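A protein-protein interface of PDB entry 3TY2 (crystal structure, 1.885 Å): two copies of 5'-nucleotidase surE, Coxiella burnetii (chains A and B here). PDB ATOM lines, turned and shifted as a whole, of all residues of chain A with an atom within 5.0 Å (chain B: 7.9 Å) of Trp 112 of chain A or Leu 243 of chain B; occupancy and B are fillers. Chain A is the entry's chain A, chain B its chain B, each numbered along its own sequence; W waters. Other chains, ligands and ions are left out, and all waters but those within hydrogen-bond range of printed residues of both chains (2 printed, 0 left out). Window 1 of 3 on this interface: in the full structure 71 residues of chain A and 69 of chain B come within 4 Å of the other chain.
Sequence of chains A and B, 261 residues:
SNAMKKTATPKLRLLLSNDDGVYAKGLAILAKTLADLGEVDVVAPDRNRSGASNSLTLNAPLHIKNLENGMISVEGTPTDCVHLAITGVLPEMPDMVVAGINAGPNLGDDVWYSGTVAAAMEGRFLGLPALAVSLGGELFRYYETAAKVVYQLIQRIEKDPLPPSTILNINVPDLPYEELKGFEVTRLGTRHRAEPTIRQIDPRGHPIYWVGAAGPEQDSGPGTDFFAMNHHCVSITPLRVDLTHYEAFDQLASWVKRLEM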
ATOM      1  N   SER A  53      33.866  27.774  -1.036  1.00  0.00           N
ATOM      2  CA  SER A  53      33.639  26.793  -2.105  1.00  0.00           C
ATOM      3  C   SER A  53      35.002  26.294  -2.576  1.00  0.00           C
ATOM      4  O   SER A  53      35.933  26.183  -1.771  1.00  0.00           O
ATOM      5  CB  SER A  53      32.863  27.437  -3.264  1.00  0.00           C
ATOM      6  OG  SER A  53      32.487  26.470  -4.233  1.00  0.00           O
ATOM      7  N   ASP A 109      22.279  21.387  -0.336  1.00  0.00           N
ATOM      8  CA  ASP A 109      22.814  22.501  -1.122  1.00  0.00           C
ATOM      9  C   ASP A 109      24.109  23.066  -0.596  1.00  0.00           C
ATOM     10  O   ASP A 109      24.875  23.664  -1.352  1.00  0.00           O
ATOM     11  CB  ASP A 109      21.819  23.658  -1.116  1.00  0.00           C
ATOM     12  CG  ASP A 109      20.597  23.366  -1.911  1.00  0.00           C
ATOM     13  OD1 ASP A 109      19.641  22.808  -1.332  1.00  0.00           O
ATOM     14  OD2 ASP A 109      20.602  23.703  -3.111  1.00  0.00           O
ATOM     15  N   ASP A 110      24.323  22.922   0.708  1.00  0.00           N
ATOM     16  CA  ASP A 110      25.476  23.526   1.363  1.00  0.00           C
ATOM     17  C   ASP A 110      26.761  23.163   0.652  1.00  0.00           C
ATOM     18  O   ASP A 110      27.705  23.951   0.631  1.00  0.00           O
ATOM     19  CB  ASP A 110      25.586  23.072   2.816  1.00  0.00           C
ATOM     20  CG  ASP A 110      24.386  23.459   3.654  1.00  0.00           C
ATOM     21  OD1 ASP A 110      23.626  24.379   3.263  1.00  0.00           O
ATOM     22  OD2 ASP A 110      24.215  22.841   4.727  1.00  0.00           O
ATOM     23  N   VAL A 111      26.812  21.963   0.082  1.00  0.00           N
ATOM     24  CA  VAL A 111      28.077  21.457  -0.438  1.00  0.00           C
ATOM     25  C   VAL A 111      28.599  22.298  -1.596  1.00  0.00           C
ATOM     26  O   VAL A 111      29.790  22.287  -1.882  1.00  0.00           O
ATOM     27  CB  VAL A 111      27.998  19.964  -0.861  1.00  0.00           C
ATOM     28  CG1 VAL A 111      27.438  19.114   0.282  1.00  0.00           C
ATOM     29  CG2 VAL A 111      27.167  19.803  -2.130  1.00  0.00           C
ATOM     30  N   TRP A 112      27.709  23.033  -2.263  1.00  0.00           N
ATOM     31  CA  TRP A 112      28.148  23.878  -3.362  1.00  0.00           C
ATOM     32  C   TRP A 112      29.059  25.000  -2.886  1.00  0.00           C
ATOM     33  O   TRP A 112      29.953  25.417  -3.613  1.00  0.00           O
ATOM     34  CB  TRP A 112      26.957  24.472  -4.129  1.00  0.00           C
ATOM     35  CG  TRP A 112      26.217  23.472  -4.968  1.00  0.00           C
ATOM     36  CD1 TRP A 112      24.967  22.980  -4.743  1.00  0.00           C
ATOM     37  CD2 TRP A 112      26.688  22.840  -6.163  1.00  0.00           C
ATOM     38  NE1 TRP A 112      24.627  22.078  -5.726  1.00  0.00           N
ATOM     39  CE2 TRP A 112      25.665  21.977  -6.612  1.00  0.00           C
ATOM     40  CE3 TRP A 112      27.873  22.917  -6.899  1.00  0.00           C
ATOM     41  CZ2 TRP A 112      25.794  21.198  -7.761  1.00  0.00           C
ATOM     42  CZ3 TRP A 112      27.999  22.140  -8.042  1.00  0.00           C
ATOM     43  CH2 TRP A 112      26.965  21.295  -8.461  1.00  0.00           C
ATOM     44  N   TYR A 113      28.836  25.476  -1.663  1.00  0.00           N
ATOM     45  CA  TYR A 113      29.536  26.666  -1.169  1.00  0.00           C
ATOM     46  C   TYR A 113      30.588  26.339  -0.119  1.00  0.00           C
ATOM     47  O   TYR A 113      31.355  27.204   0.287  1.00  0.00           O
ATOM     48  CB  TYR A 113      28.528  27.627  -0.543  1.00  0.00           C
ATOM     49  CG  TYR A 113      27.264  27.768  -1.358  1.00  0.00           C
ATOM     50  CD1 TYR A 113      27.242  28.542  -2.513  1.00  0.00           C
ATOM     51  CD2 TYR A 113      26.101  27.116  -0.981  1.00  0.00           C
ATOM     52  CE1 TYR A 113      26.082  28.663  -3.273  1.00  0.00           C
ATOM     53  CE2 TYR A 113      24.943  27.231  -1.726  1.00  0.00           C
ATOM     54  CZ  TYR A 113      24.938  28.002  -2.868  1.00  0.00           C
ATOM     55  OH  TYR A 113      23.779  28.116  -3.606  1.00  0.00           O
ATOM     56  N   SER A 114      30.605  25.094   0.335  1.00  0.00           N
ATOM     57  CA  SER A 114      31.424  24.717   1.484  1.00  0.00           C
ATOM     58  C   SER A 114      32.916  24.638   1.170  1.00  0.00           C
ATOM     59  O   SER A 114      33.330  23.882   0.289  1.00  0.00           O
ATOM     60  CB  SER A 114      30.955  23.377   2.049  1.00  0.00           C
ATOM     61  OG  SER A 114      31.888  22.898   3.011  1.00  0.00           O
ATOM     62  N   LEU A 188      22.231  13.690  -1.114  1.00  0.00           N
ATOM     63  CA  LEU A 188      22.064  15.099  -0.782  1.00  0.00           C
ATOM     64  C   LEU A 188      20.603  15.516  -0.809  1.00  0.00           C
ATOM     65  O   LEU A 188      19.915  15.342  -1.812  1.00  0.00           O
ATOM     66  CB  LEU A 188      22.842  15.972  -1.769  1.00  0.00           C
ATOM     67  CG  LEU A 188      24.353  15.770  -1.802  1.00  0.00           C
ATOM     68  CD1 LEU A 188      24.955  16.617  -2.914  1.00  0.00           C
ATOM     69  CD2 LEU A 188      24.958  16.133  -0.459  1.00  0.00           C
ATOM     70  N   PRO A 238      28.498   9.920  -0.636  1.00  0.00           N
ATOM     71  CA  PRO A 238      29.606   9.922  -1.590  1.00  0.00           C
ATOM     72  C   PRO A 238      29.327  10.990  -2.641  1.00  0.00           C
ATOM     73  O   PRO A 238      28.189  11.100  -3.118  1.00  0.00           O
ATOM     74  CB  PRO A 238      29.518   8.530  -2.215  1.00  0.00           C
ATOM     75  CG  PRO A 238      28.049   8.218  -2.183  1.00  0.00           C
ATOM     76  CD  PRO A 238      27.498   8.882  -0.941  1.00  0.00           C
ATOM     77  N   LEU A 239      30.343  11.775  -2.986  1.00  0.00           N
ATOM     78  CA  LEU A 239      30.175  12.852  -3.953  1.00  0.00           C
ATOM     79  C   LEU A 239      30.868  12.513  -5.274  1.00  0.00           C
ATOM     80  O   LEU A 239      31.913  11.874  -5.290  1.00  0.00           O
ATOM     81  CB  LEU A 239      30.733  14.155  -3.375  1.00  0.00           C
ATOM     82  CG  LEU A 239      30.065  14.643  -2.087  1.00  0.00           C
ATOM     83  CD1 LEU A 239      30.739  15.910  -1.553  1.00  0.00           C
ATOM     84  CD2 LEU A 239      28.563  14.868  -2.290  1.00  0.00           C
ATOM     85  N   ARG A 240      30.308  12.970  -6.387  1.00  0.00           N
ATOM     86  CA  ARG A 240      30.870  12.602  -7.680  1.00  0.00           C
ATOM     87  C   ARG A 240      31.802  13.663  -8.233  1.00  0.00           C
ATOM     88  O   ARG A 240      31.734  14.829  -7.848  1.00  0.00           O
ATOM     89  CB  ARG A 240      29.761  12.306  -8.681  1.00  0.00           C
ATOM     90  CG  ARG A 240      28.812  13.457  -8.893  1.00  0.00           C
ATOM     91  CD  ARG A 240      27.542  12.944  -9.517  1.00  0.00           C
ATOM     92  NE  ARG A 240      27.833  12.112 -10.682  1.00  0.00           N
ATOM     93  CZ  ARG A 240      27.047  11.131 -11.110  1.00  0.00           C
ATOM     94  NH1 ARG A 240      25.922  10.854 -10.463  1.00  0.00           N
ATOM     95  NH2 ARG A 240      27.385  10.425 -12.179  1.00  0.00           N
ATOM     96  N   LEU A 243      30.790  16.213 -13.454  1.00  0.00           N
ATOM     97  CA  LEU A 243      29.712  17.196 -13.432  1.00  0.00           C
ATOM     98  C   LEU A 243      28.810  17.111 -14.657  1.00  0.00           C
ATOM     99  O   LEU A 243      27.765  17.769 -14.719  1.00  0.00           O
ATOM    100  CB  LEU A 243      30.317  18.597 -13.350  1.00  0.00           C
ATOM    101  CG  LEU A 243      29.460  19.759 -12.852  1.00  0.00           C
ATOM    102  CD1 LEU A 243      29.008  19.512 -11.421  1.00  0.00           C
ATOM    103  CD2 LEU A 243      30.262  21.057 -12.941  1.00  0.00           C
ATOM    104  N   ALA B  52      36.823  32.380  -8.722  1.00  0.00           N
ATOM    105  CA  ALA B  52      35.926  32.522  -7.567  1.00  0.00           C
ATOM    106  C   ALA B  52      35.050  31.285  -7.335  1.00  0.00           C
ATOM    107  O   ALA B  52      34.541  31.066  -6.231  1.00  0.00           O
ATOM    108  CB  ALA B  52      35.052  33.766  -7.717  1.00  0.00           C
ATOM    109  N   SER B  53      34.855  30.487  -8.383  1.00  0.00           N
ATOM    110  CA  SER B  53      34.002  29.308  -8.276  1.00  0.00           C
ATOM    111  C   SER B  53      32.656  29.731  -7.699  1.00  0.00           C
ATOM    112  O   SER B  53      32.174  30.817  -8.012  1.00  0.00           O
ATOM    113  CB  SER B  53      34.657  28.249  -7.394  1.00  0.00           C
ATOM    114  OG  SER B  53      33.949  27.022  -7.456  1.00  0.00           O
ATOM    115  N   ASN B  54      32.062  28.885  -6.859  1.00  0.00           N
ATOM    116  CA  ASN B  54      30.769  29.196  -6.248  1.00  0.00           C
ATOM    117  C   ASN B  54      30.939  29.897  -4.897  1.00  0.00           C
ATOM    118  O   ASN B  54      30.062  29.807  -4.041  1.00  0.00           O
ATOM    119  CB  ASN B  54      29.937  27.926  -6.036  1.00  0.00           C
ATOM    120  CG  ASN B  54      29.800  27.086  -7.305  1.00  0.00           C
ATOM    121  OD1 ASN B  54      30.777  26.516  -7.790  1.00  0.00           O
ATOM    122  ND2 ASN B  54      28.581  26.992  -7.832  1.00  0.00           N
ATOM    123  N   SER B  55      32.072  30.562  -4.692  1.00  0.00           N
ATOM    124  CA  SER B  55      32.313  31.210  -3.396  1.00  0.00           C
ATOM    125  C   SER B  55      31.265  32.274  -3.073  1.00  0.00           C
ATOM    126  O   SER B  55      30.827  33.015  -3.947  1.00  0.00           O
ATOM    127  CB  SER B  55      33.721  31.808  -3.306  1.00  0.00           C
ATOM    128  OG  SER B  55      33.955  32.781  -4.312  1.00  0.00           O
ATOM    129  N   LEU B  56      30.868  32.313  -1.803  1.00  0.00           N
ATOM    130  CA  LEU B  56      29.971  33.332  -1.282  1.00  0.00           C
ATOM    131  C   LEU B  56      30.708  34.112  -0.210  1.00  0.00           C
ATOM    132  O   LEU B  56      31.506  33.550   0.547  1.00  0.00           O
ATOM    133  CB  LEU B  56      28.727  32.697  -0.650  1.00  0.00           C
ATOM    134  CG  LEU B  56      27.552  32.207  -1.490  1.00  0.00           C
ATOM    135  CD1 LEU B  56      26.557  31.466  -0.598  1.00  0.00           C
ATOM    136  CD2 LEU B  56      26.863  33.381  -2.205  1.00  0.00           C
ATOM    137  N   THR B  79      28.794  34.516  -7.548  1.00  0.00           N
ATOM    138  CA  THR B  79      27.718  33.815  -6.867  1.00  0.00           C
ATOM    139  C   THR B  79      26.998  34.770  -5.920  1.00  0.00           C
ATOM    140  O   THR B  79      25.773  34.724  -5.819  1.00  0.00           O
ATOM    141  CB  THR B  79      28.228  32.555  -6.137  1.00  0.00           C
ATOM    142  OG1 THR B  79      28.816  31.666  -7.106  1.00  0.00           O
ATOM    143  CG2 THR B  79      27.089  31.828  -5.425  1.00  0.00           C
ATOM    144  N   VAL B 111      35.786  24.070 -15.406  1.00  0.00           N
ATOM    145  CA  VAL B 111      34.437  24.479 -15.013  1.00  0.00           C
ATOM    146  C   VAL B 111      34.214  24.388 -13.512  1.00  0.00           C
ATOM    147  O   VAL B 111      33.372  25.085 -12.969  1.00  0.00           O
ATOM    148  CB  VAL B 111      33.335  23.667 -15.736  1.00  0.00           C
ATOM    149  CG1 VAL B 111      33.626  23.589 -17.225  1.00  0.00           C
ATOM    150  CG2 VAL B 111      33.196  22.283 -15.116  1.00  0.00           C
ATOM    151  N   TRP B 112      34.978  23.539 -12.836  1.00  0.00           N
ATOM    152  CA  TRP B 112      34.851  23.397 -11.395  1.00  0.00           C
ATOM    153  C   TRP B 112      35.231  24.669 -10.625  1.00  0.00           C
ATOM    154  O   TRP B 112      34.756  24.899  -9.514  1.00  0.00           O
ATOM    155  CB  TRP B 112      35.696  22.214 -10.916  1.00  0.00           C
ATOM    156  CG  TRP B 112      35.025  20.903 -11.173  1.00  0.00           C
ATOM    157  CD1 TRP B 112      34.940  20.241 -12.364  1.00  0.00           C
ATOM    158  CD2 TRP B 112      34.313  20.107 -10.220  1.00  0.00           C
ATOM    159  NE1 TRP B 112      34.226  19.075 -12.208  1.00  0.00           N
ATOM    160  CE2 TRP B 112      33.833  18.970 -10.899  1.00  0.00           C
ATOM    161  CE3 TRP B 112      34.044  20.242  -8.857  1.00  0.00           C
ATOM    162  CZ2 TRP B 112      33.097  17.978 -10.261  1.00  0.00           C
ATOM    163  CZ3 TRP B 112      33.313  19.257  -8.225  1.00  0.00           C
ATOM    164  CH2 TRP B 112      32.849  18.138  -8.926  1.00  0.00           C
ATOM    165  N   VAL B 117      30.524  29.875 -14.574  1.00  0.00           N
ATOM    166  CA  VAL B 117      29.681  28.706 -14.433  1.00  0.00           C
ATOM    167  C   VAL B 117      28.915  28.767 -13.113  1.00  0.00           C
ATOM    168  O   VAL B 117      27.733  28.429 -13.060  1.00  0.00           O
ATOM    169  CB  VAL B 117      30.500  27.392 -14.507  1.00  0.00           C
ATOM    170  CG1 VAL B 117      29.607  26.196 -14.207  1.00  0.00           C
ATOM    171  CG2 VAL B 117      31.149  27.242 -15.871  1.00  0.00           C
ATOM    172  N   ALA B 118      29.582  29.211 -12.048  1.00  0.00           N
ATOM    173  CA  ALA B 118      28.955  29.259 -10.727  1.00  0.00           C
ATOM    174  C   ALA B 118      27.750  30.203 -10.693  1.00  0.00           C
ATOM    175  O   ALA B 118      26.723  29.890 -10.083  1.00  0.00           O
ATOM    176  CB  ALA B 118      29.978  29.663  -9.651  1.00  0.00           C
ATOM    177  N   MET B 121      24.912  28.353 -12.202  1.00  0.00           N
ATOM    178  CA  MET B 121      24.472  27.327 -11.256  1.00  0.00           C
ATOM    179  C   MET B 121      23.563  27.903 -10.165  1.00  0.00           C
ATOM    180  O   MET B 121      22.637  27.239  -9.694  1.00  0.00           O
ATOM    181  CB  MET B 121      25.692  26.633 -10.641  1.00  0.00           C
ATOM    182  CG  MET B 121      25.376  25.520  -9.662  1.00  0.00           C
ATOM    183  SD  MET B 121      24.418  24.020 -10.495  1.00  0.00           S
ATOM    184  CE  MET B 121      25.833  23.388 -11.673  1.00  0.00           C
ATOM    185  N   GLU B 122      23.829  29.142  -9.761  1.00  0.00           N
ATOM    186  CA  GLU B 122      23.009  29.799  -8.742  1.00  0.00           C
ATOM    187  C   GLU B 122      21.604  30.095  -9.281  1.00  0.00           C
ATOM    188  O   GLU B 122      20.649  30.254  -8.513  1.00  0.00           O
ATOM    189  CB  GLU B 122      23.701  31.066  -8.207  1.00  0.00           C
ATOM    190  CG  GLU B 122      23.159  31.586  -6.880  1.00  0.00           C
ATOM    191  CD  GLU B 122      23.398  30.631  -5.713  1.00  0.00           C
ATOM    192  OE1 GLU B 122      24.151  29.648  -5.876  1.00  0.00           O
ATOM    193  OE2 GLU B 122      22.822  30.864  -4.634  1.00  0.00           O
ATOM    194  N   ARG B 124      19.790  27.959 -10.719  1.00  0.00           N
ATOM    195  CA  ARG B 124      19.040  26.706 -10.732  1.00  0.00           C
ATOM    196  C   ARG B 124      17.751  26.849  -9.927  1.00  0.00           C
ATOM    197  O   ARG B 124      16.787  26.133 -10.166  1.00  0.00           O
ATOM    198  CB  ARG B 124      19.887  25.540 -10.187  1.00  0.00           C
ATOM    199  CG  ARG B 124      20.128  25.572  -8.678  1.00  0.00           C
ATOM    200  CD  ARG B 124      21.214  24.577  -8.242  1.00  0.00           C
ATOM    201  NE  ARG B 124      21.481  24.683  -6.808  1.00  0.00           N
ATOM    202  CZ  ARG B 124      22.317  25.571  -6.272  1.00  0.00           C
ATOM    203  NH1 ARG B 124      22.978  26.413  -7.053  1.00  0.00           N
ATOM    204  NH2 ARG B 124      22.501  25.616  -4.957  1.00  0.00           N
ATOM    205  N   PHE B 125      17.737  27.783  -8.979  1.00  0.00           N
ATOM    206  CA  PHE B 125      16.541  28.030  -8.170  1.00  0.00           C
ATOM    207  C   PHE B 125      15.383  28.635  -8.977  1.00  0.00           C
ATOM    208  O   PHE B 125      14.244  28.612  -8.524  1.00  0.00           O
ATOM    209  CB  PHE B 125      16.852  28.950  -6.976  1.00  0.00           C
ATOM    210  CG  PHE B 125      17.892  28.409  -6.031  1.00  0.00           C
ATOM    211  CD1 PHE B 125      17.552  27.483  -5.059  1.00  0.00           C
ATOM    212  CD2 PHE B 125      19.207  28.843  -6.104  1.00  0.00           C
ATOM    213  CE1 PHE B 125      18.505  26.987  -4.188  1.00  0.00           C
ATOM    214  CE2 PHE B 125      20.166  28.354  -5.227  1.00  0.00           C
ATOM    215  CZ  PHE B 125      19.816  27.424  -4.273  1.00  0.00           C
ATOM    216  N   ILE B 167      21.052  23.397 -16.344  1.00  0.00           N
ATOM    217  CA  ILE B 167      22.139  24.371 -16.363  1.00  0.00           C
ATOM    218  C   ILE B 167      23.041  24.027 -17.533  1.00  0.00           C
ATOM    219  O   ILE B 167      23.626  22.938 -17.563  1.00  0.00           O
ATOM    220  CB  ILE B 167      22.997  24.309 -15.068  1.00  0.00           C
ATOM    221  CG1 ILE B 167      22.122  24.322 -13.806  1.00  0.00           C
ATOM    222  CG2 ILE B 167      24.037  25.423 -15.046  1.00  0.00           C
ATOM    223  CD1 ILE B 167      21.114  25.457 -13.737  1.00  0.00           C
ATOM    224  N   LEU B 239      24.902  20.464 -16.989  1.00  0.00           N
ATOM    225  CA  LEU B 239      25.617  20.195 -15.742  1.00  0.00           C
ATOM    226  C   LEU B 239      24.712  19.648 -14.648  1.00  0.00           C
ATOM    227  O   LEU B 239      23.556  20.058 -14.519  1.00  0.00           O
ATOM    228  CB  LEU B 239      26.318  21.457 -15.235  1.00  0.00           C
ATOM    229  CG  LEU B 239      27.322  22.086 -16.203  1.00  0.00           C
ATOM    230  CD1 LEU B 239      27.884  23.396 -15.633  1.00  0.00           C
ATOM    231  CD2 LEU B 239      28.440  21.102 -16.513  1.00  0.00           C
ATOM    232  N   ARG B 240      25.254  18.741 -13.841  1.00  0.00           N
ATOM    233  CA  ARG B 240      24.489  18.141 -12.758  1.00  0.00           C
ATOM    234  C   ARG B 240      24.214  19.159 -11.666  1.00  0.00           C
ATOM    235  O   ARG B 240      25.076  19.977 -11.342  1.00  0.00           O
ATOM    236  CB  ARG B 240      25.247  16.958 -12.152  1.00  0.00           C
ATOM    237  CG  ARG B 240      25.543  15.836 -13.124  1.00  0.00           C
ATOM    238  CD  ARG B 240      26.128  14.650 -12.385  1.00  0.00           C
ATOM    239  NE  ARG B 240      26.601  13.609 -13.293  1.00  0.00           N
ATOM    240  CZ  ARG B 240      25.849  12.612 -13.746  1.00  0.00           C
ATOM    241  NH1 ARG B 240      24.577  12.514 -13.383  1.00  0.00           N
ATOM    242  NH2 ARG B 240      26.373  11.712 -14.566  1.00  0.00           N
ATOM    243  N   VAL B 241      23.019  19.098 -11.085  1.00  0.00           N
ATOM    244  CA  VAL B 241      22.719  19.919  -9.913  1.00  0.00           C
ATOM    245  C   VAL B 241      22.677  19.071  -8.641  1.00  0.00           C
ATOM    246  O   VAL B 241      22.503  19.585  -7.534  1.00  0.00           O
ATOM    247  CB  VAL B 241      21.402  20.708 -10.081  1.00  0.00           C
ATOM    248  CG1 VAL B 241      21.510  21.676 -11.262  1.00  0.00           C
ATOM    249  CG2 VAL B 241      20.233  19.752 -10.273  1.00  0.00           C
ATOM    250  N   ASP B 242      22.853  17.766  -8.809  1.00  0.00           N
ATOM    251  CA  ASP B 242      22.914  16.837  -7.686  1.00  0.00           C
ATOM    252  C   ASP B 242      24.272  16.132  -7.707  1.00  0.00           C
ATOM    253  O   ASP B 242      24.574  15.368  -8.629  1.00  0.00           O
ATOM    254  CB  ASP B 242      21.782  15.817  -7.797  1.00  0.00           C
ATOM    255  CG  ASP B 242      21.744  14.841  -6.629  1.00  0.00           C
ATOM    256  OD1 ASP B 242      22.634  14.905  -5.757  1.00  0.00           O
ATOM    257  OD2 ASP B 242      20.823  14.002  -6.595  1.00  0.00           O
ATOM    258  N   LEU B 243      25.085  16.401  -6.695  1.00  0.00           N
ATOM    259  CA  LEU B 243      26.443  15.863  -6.608  1.00  0.00           C
ATOM    260  C   LEU B 243      26.528  14.471  -5.966  1.00  0.00           C
ATOM    261  O   LEU B 243      27.617  13.927  -5.787  1.00  0.00           O
ATOM    262  CB  LEU B 243      27.334  16.838  -5.839  1.00  0.00           C
ATOM    263  CG  LEU B 243      27.427  18.240  -6.442  1.00  0.00           C
ATOM    264  CD1 LEU B 243      28.079  19.218  -5.467  1.00  0.00           C
ATOM    265  CD2 LEU B 243      28.187  18.184  -7.754  1.00  0.00           C
ATOM    266  N   THR B 244      25.382  13.896  -5.627  1.00  0.00           N
ATOM    267  CA  THR B 244      25.347  12.535  -5.083  1.00  0.00           C
ATOM    268  C   THR B 244      25.868  11.499  -6.083  1.00  0.00           C
ATOM    269  O   THR B 244      25.403  11.436  -7.221  1.00  0.00           O
ATOM    270  CB  THR B 244      23.919  12.143  -4.665  1.00  0.00           C
ATOM    271  OG1 THR B 244      23.391  13.125  -3.768  1.00  0.00           O
ATOM    272  CG2 THR B 244      23.919  10.773  -3.983  1.00  0.00           C
ATOM    273  N   HIS B 245      26.828  10.674  -5.662  1.00  0.00           N
ATOM    274  CA  HIS B 245      27.404   9.667  -6.551  1.00  0.00           C
ATOM    275  C   HIS B 245      26.629   8.356  -6.399  1.00  0.00           C
ATOM    276  O   HIS B 245      27.042   7.454  -5.665  1.00  0.00           O
ATOM    277  CB  HIS B 245      28.888   9.453  -6.245  1.00  0.00           C
ATOM    278  CG  HIS B 245      29.621   8.666  -7.289  1.00  0.00           C
ATOM    279  ND1 HIS B 245      30.938   8.282  -7.138  1.00  0.00           N
ATOM    280  CD2 HIS B 245      29.240   8.207  -8.505  1.00  0.00           C
ATOM    281  CE1 HIS B 245      31.328   7.613  -8.204  1.00  0.00           C
ATOM    282  NE2 HIS B 245      30.314   7.550  -9.052  1.00  0.00           N
ATOM    283  N   TYR B 246      25.493   8.262  -7.079  1.00  0.00           N
ATOM    284  CA  TYR B 246      24.614   7.105  -6.927  1.00  0.00           C
ATOM    285  C   TYR B 246      25.296   5.790  -7.310  1.00  0.00           C
ATOM    286  O   TYR B 246      25.033   4.748  -6.710  1.00  0.00           O
ATOM    287  CB  TYR B 246      23.306   7.307  -7.703  1.00  0.00           C
ATOM    288  CG  TYR B 246      22.484   8.452  -7.156  1.00  0.00           C
ATOM    289  CD1 TYR B 246      22.445   9.685  -7.800  1.00  0.00           C
ATOM    290  CD2 TYR B 246      21.769   8.307  -5.976  1.00  0.00           C
ATOM    291  CE1 TYR B 246      21.700  10.738  -7.285  1.00  0.00           C
ATOM    292  CE2 TYR B 246      21.027   9.347  -5.454  1.00  0.00           C
ATOM    293  CZ  TYR B 246      20.996  10.562  -6.109  1.00  0.00           C
ATOM    294  OH  TYR B 246      20.248  11.590  -5.582  1.00  0.00           O
HETATM  295  O   HOH W   1      24.171  12.771  -9.141  1.00  0.00           O
HETATM  296  O   HOH W   2      33.675  16.822 -14.046  1.00  0.00           O
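The guanidinium group of Arg 124 of chain B is in salt-bridge range of the side-chain carboxylate of Asp 109 of chain A (3.3 Å).
OH of Tyr 113 of chain A sits at hydrogen-bond distance from OE1 of Glu 122 of chain B.
OH of Tyr 113 of chain A lies within hydrogen-bond range of NH2 of Arg 124 of chain B (3.1 Å).
N of Leu 188 of chain A is in hydrogen-bond range of OG1 of Thr 244 of chain B.
The backbone carbonyl oxygen (O) of Pro 238 of chain A lies within hydrogen-bond range of the backbone NH (N) of His 245 of chain B (2.9 Å).
N of Arg 240 of chain A sits at hydrogen-bond distance from O of Leu 243 of chain B.
The guanidinium group (NH1) of Arg 240 of chain A lies within hydrogen-bond range of the backbone carbonyl oxygen (O) of Thr 244 of chain B (3.3 Å).
The backbone carbonyl oxygen of Leu 243 of chain A sits at hydrogen-bond distance from the backbone NH of Arg 240 of chain B (2.8 Å).
The guanidinium group (NH2) of Arg 240 of chain A sits close to the guanidinium group (NH2) of Arg 240 of chain B (2.9 Å).
The backbone carbonyl oxygen (O) of Ala 52 of chain B lies within hydrogen-bond range of the side-chain hydroxyl (OG) of Ser 55 of chain B (2.6 Å).
The backbone carbonyl oxygen (O) of Met 121 of chain B sits at hydrogen-bond distance from the guanidinium group (NH1) of Arg 124 of chain B, 2.8 Å away.
Trp 112 of chain A touches Asn 54 of chain B.
Met 121 of chain B touches Trp 112 of chain A.
NH2 of Arg 124 of chain B touches CD1 of Trp 112 of chain A (3.6 Å).
Tyr 113 of chain A touches Thr 79 of chain B.
Leu 243 of chain B touches Leu 188 of chain A (CB to CD1, 3.8 Å).
Pro 238 of chain A touches Leu 243 of chain B.
CB of His 245 of chain B touches C of Leu 239 of chain A, 3.8 Å away.
Trp 112 of chain B touches Arg 240 of chain A.
Printed residues of chain B within 4 Å of Ser 53 of chain A: Ser 53, Asn 54 and Ser 55.
Printed residues of chain B within 4 Å of Trp 112 of chain A: Asn 54 (3.5 Å), Met 121 (3.997 Å), Arg 124 (3.6 Å), Arg 240 (3.7 Å), Val 241 (3.7 Å) and Leu 243 (3.4 Å).
Ile 167 of chain B touches none of the printed residues of chain A.
The nearest printed residue of chain B that does not touch Trp 112 of chain A is Asp 242 of chain B (4.6 Å).
Of the 12 printed residues of chain A, 10 touch a printed residue of chain B.
Printed residues of chain A that touch a printed residue of chain B: Ser 53, Asp 109, Val 111, Trp 112, Tyr 113, Leu 188, Pro 238, Leu 239, Arg 240 and Leu 243.
Hydrophobic or aromatic side chains of chain A within 4 Å of the printed part of chain B: Val 111, Trp 112, Tyr 113, Leu 188, Pro 238, Leu 239 and Leu 243.
Hydrophobic or aromatic side chains of chain B that line the printed part of chain A: Leu 56, Val 111, Trp 112, Met 121, Phe 125, Leu 239, Leu 243 and His 245.
Along chain B the printed residues that touch a printed residue of chain A span positions 53 to 245.
Leu 239 of chain A touches Leu 243 of chain B, and with the chains exchanged Leu 243 of chain A touches Leu 239 of chain B.
Arg 240 of chain A touches Leu 243 of chain B, and with the chains exchanged Leu 243 of chain A touches Arg 240 of chain B.
Leu 243 of chain A touches its own counterpart, Leu 243 of chain B.
Water W1 lies within hydrogen-bond range of O of Thr 244 of chain B, O of Asp 242 of chain B and NH1 of Arg 240 of chain A.
Water W2 lies within hydrogen-bond range of NE1 of Trp 112 of chain B (3.0 Å) and N of Leu 243 of chain A (3.0 Å).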
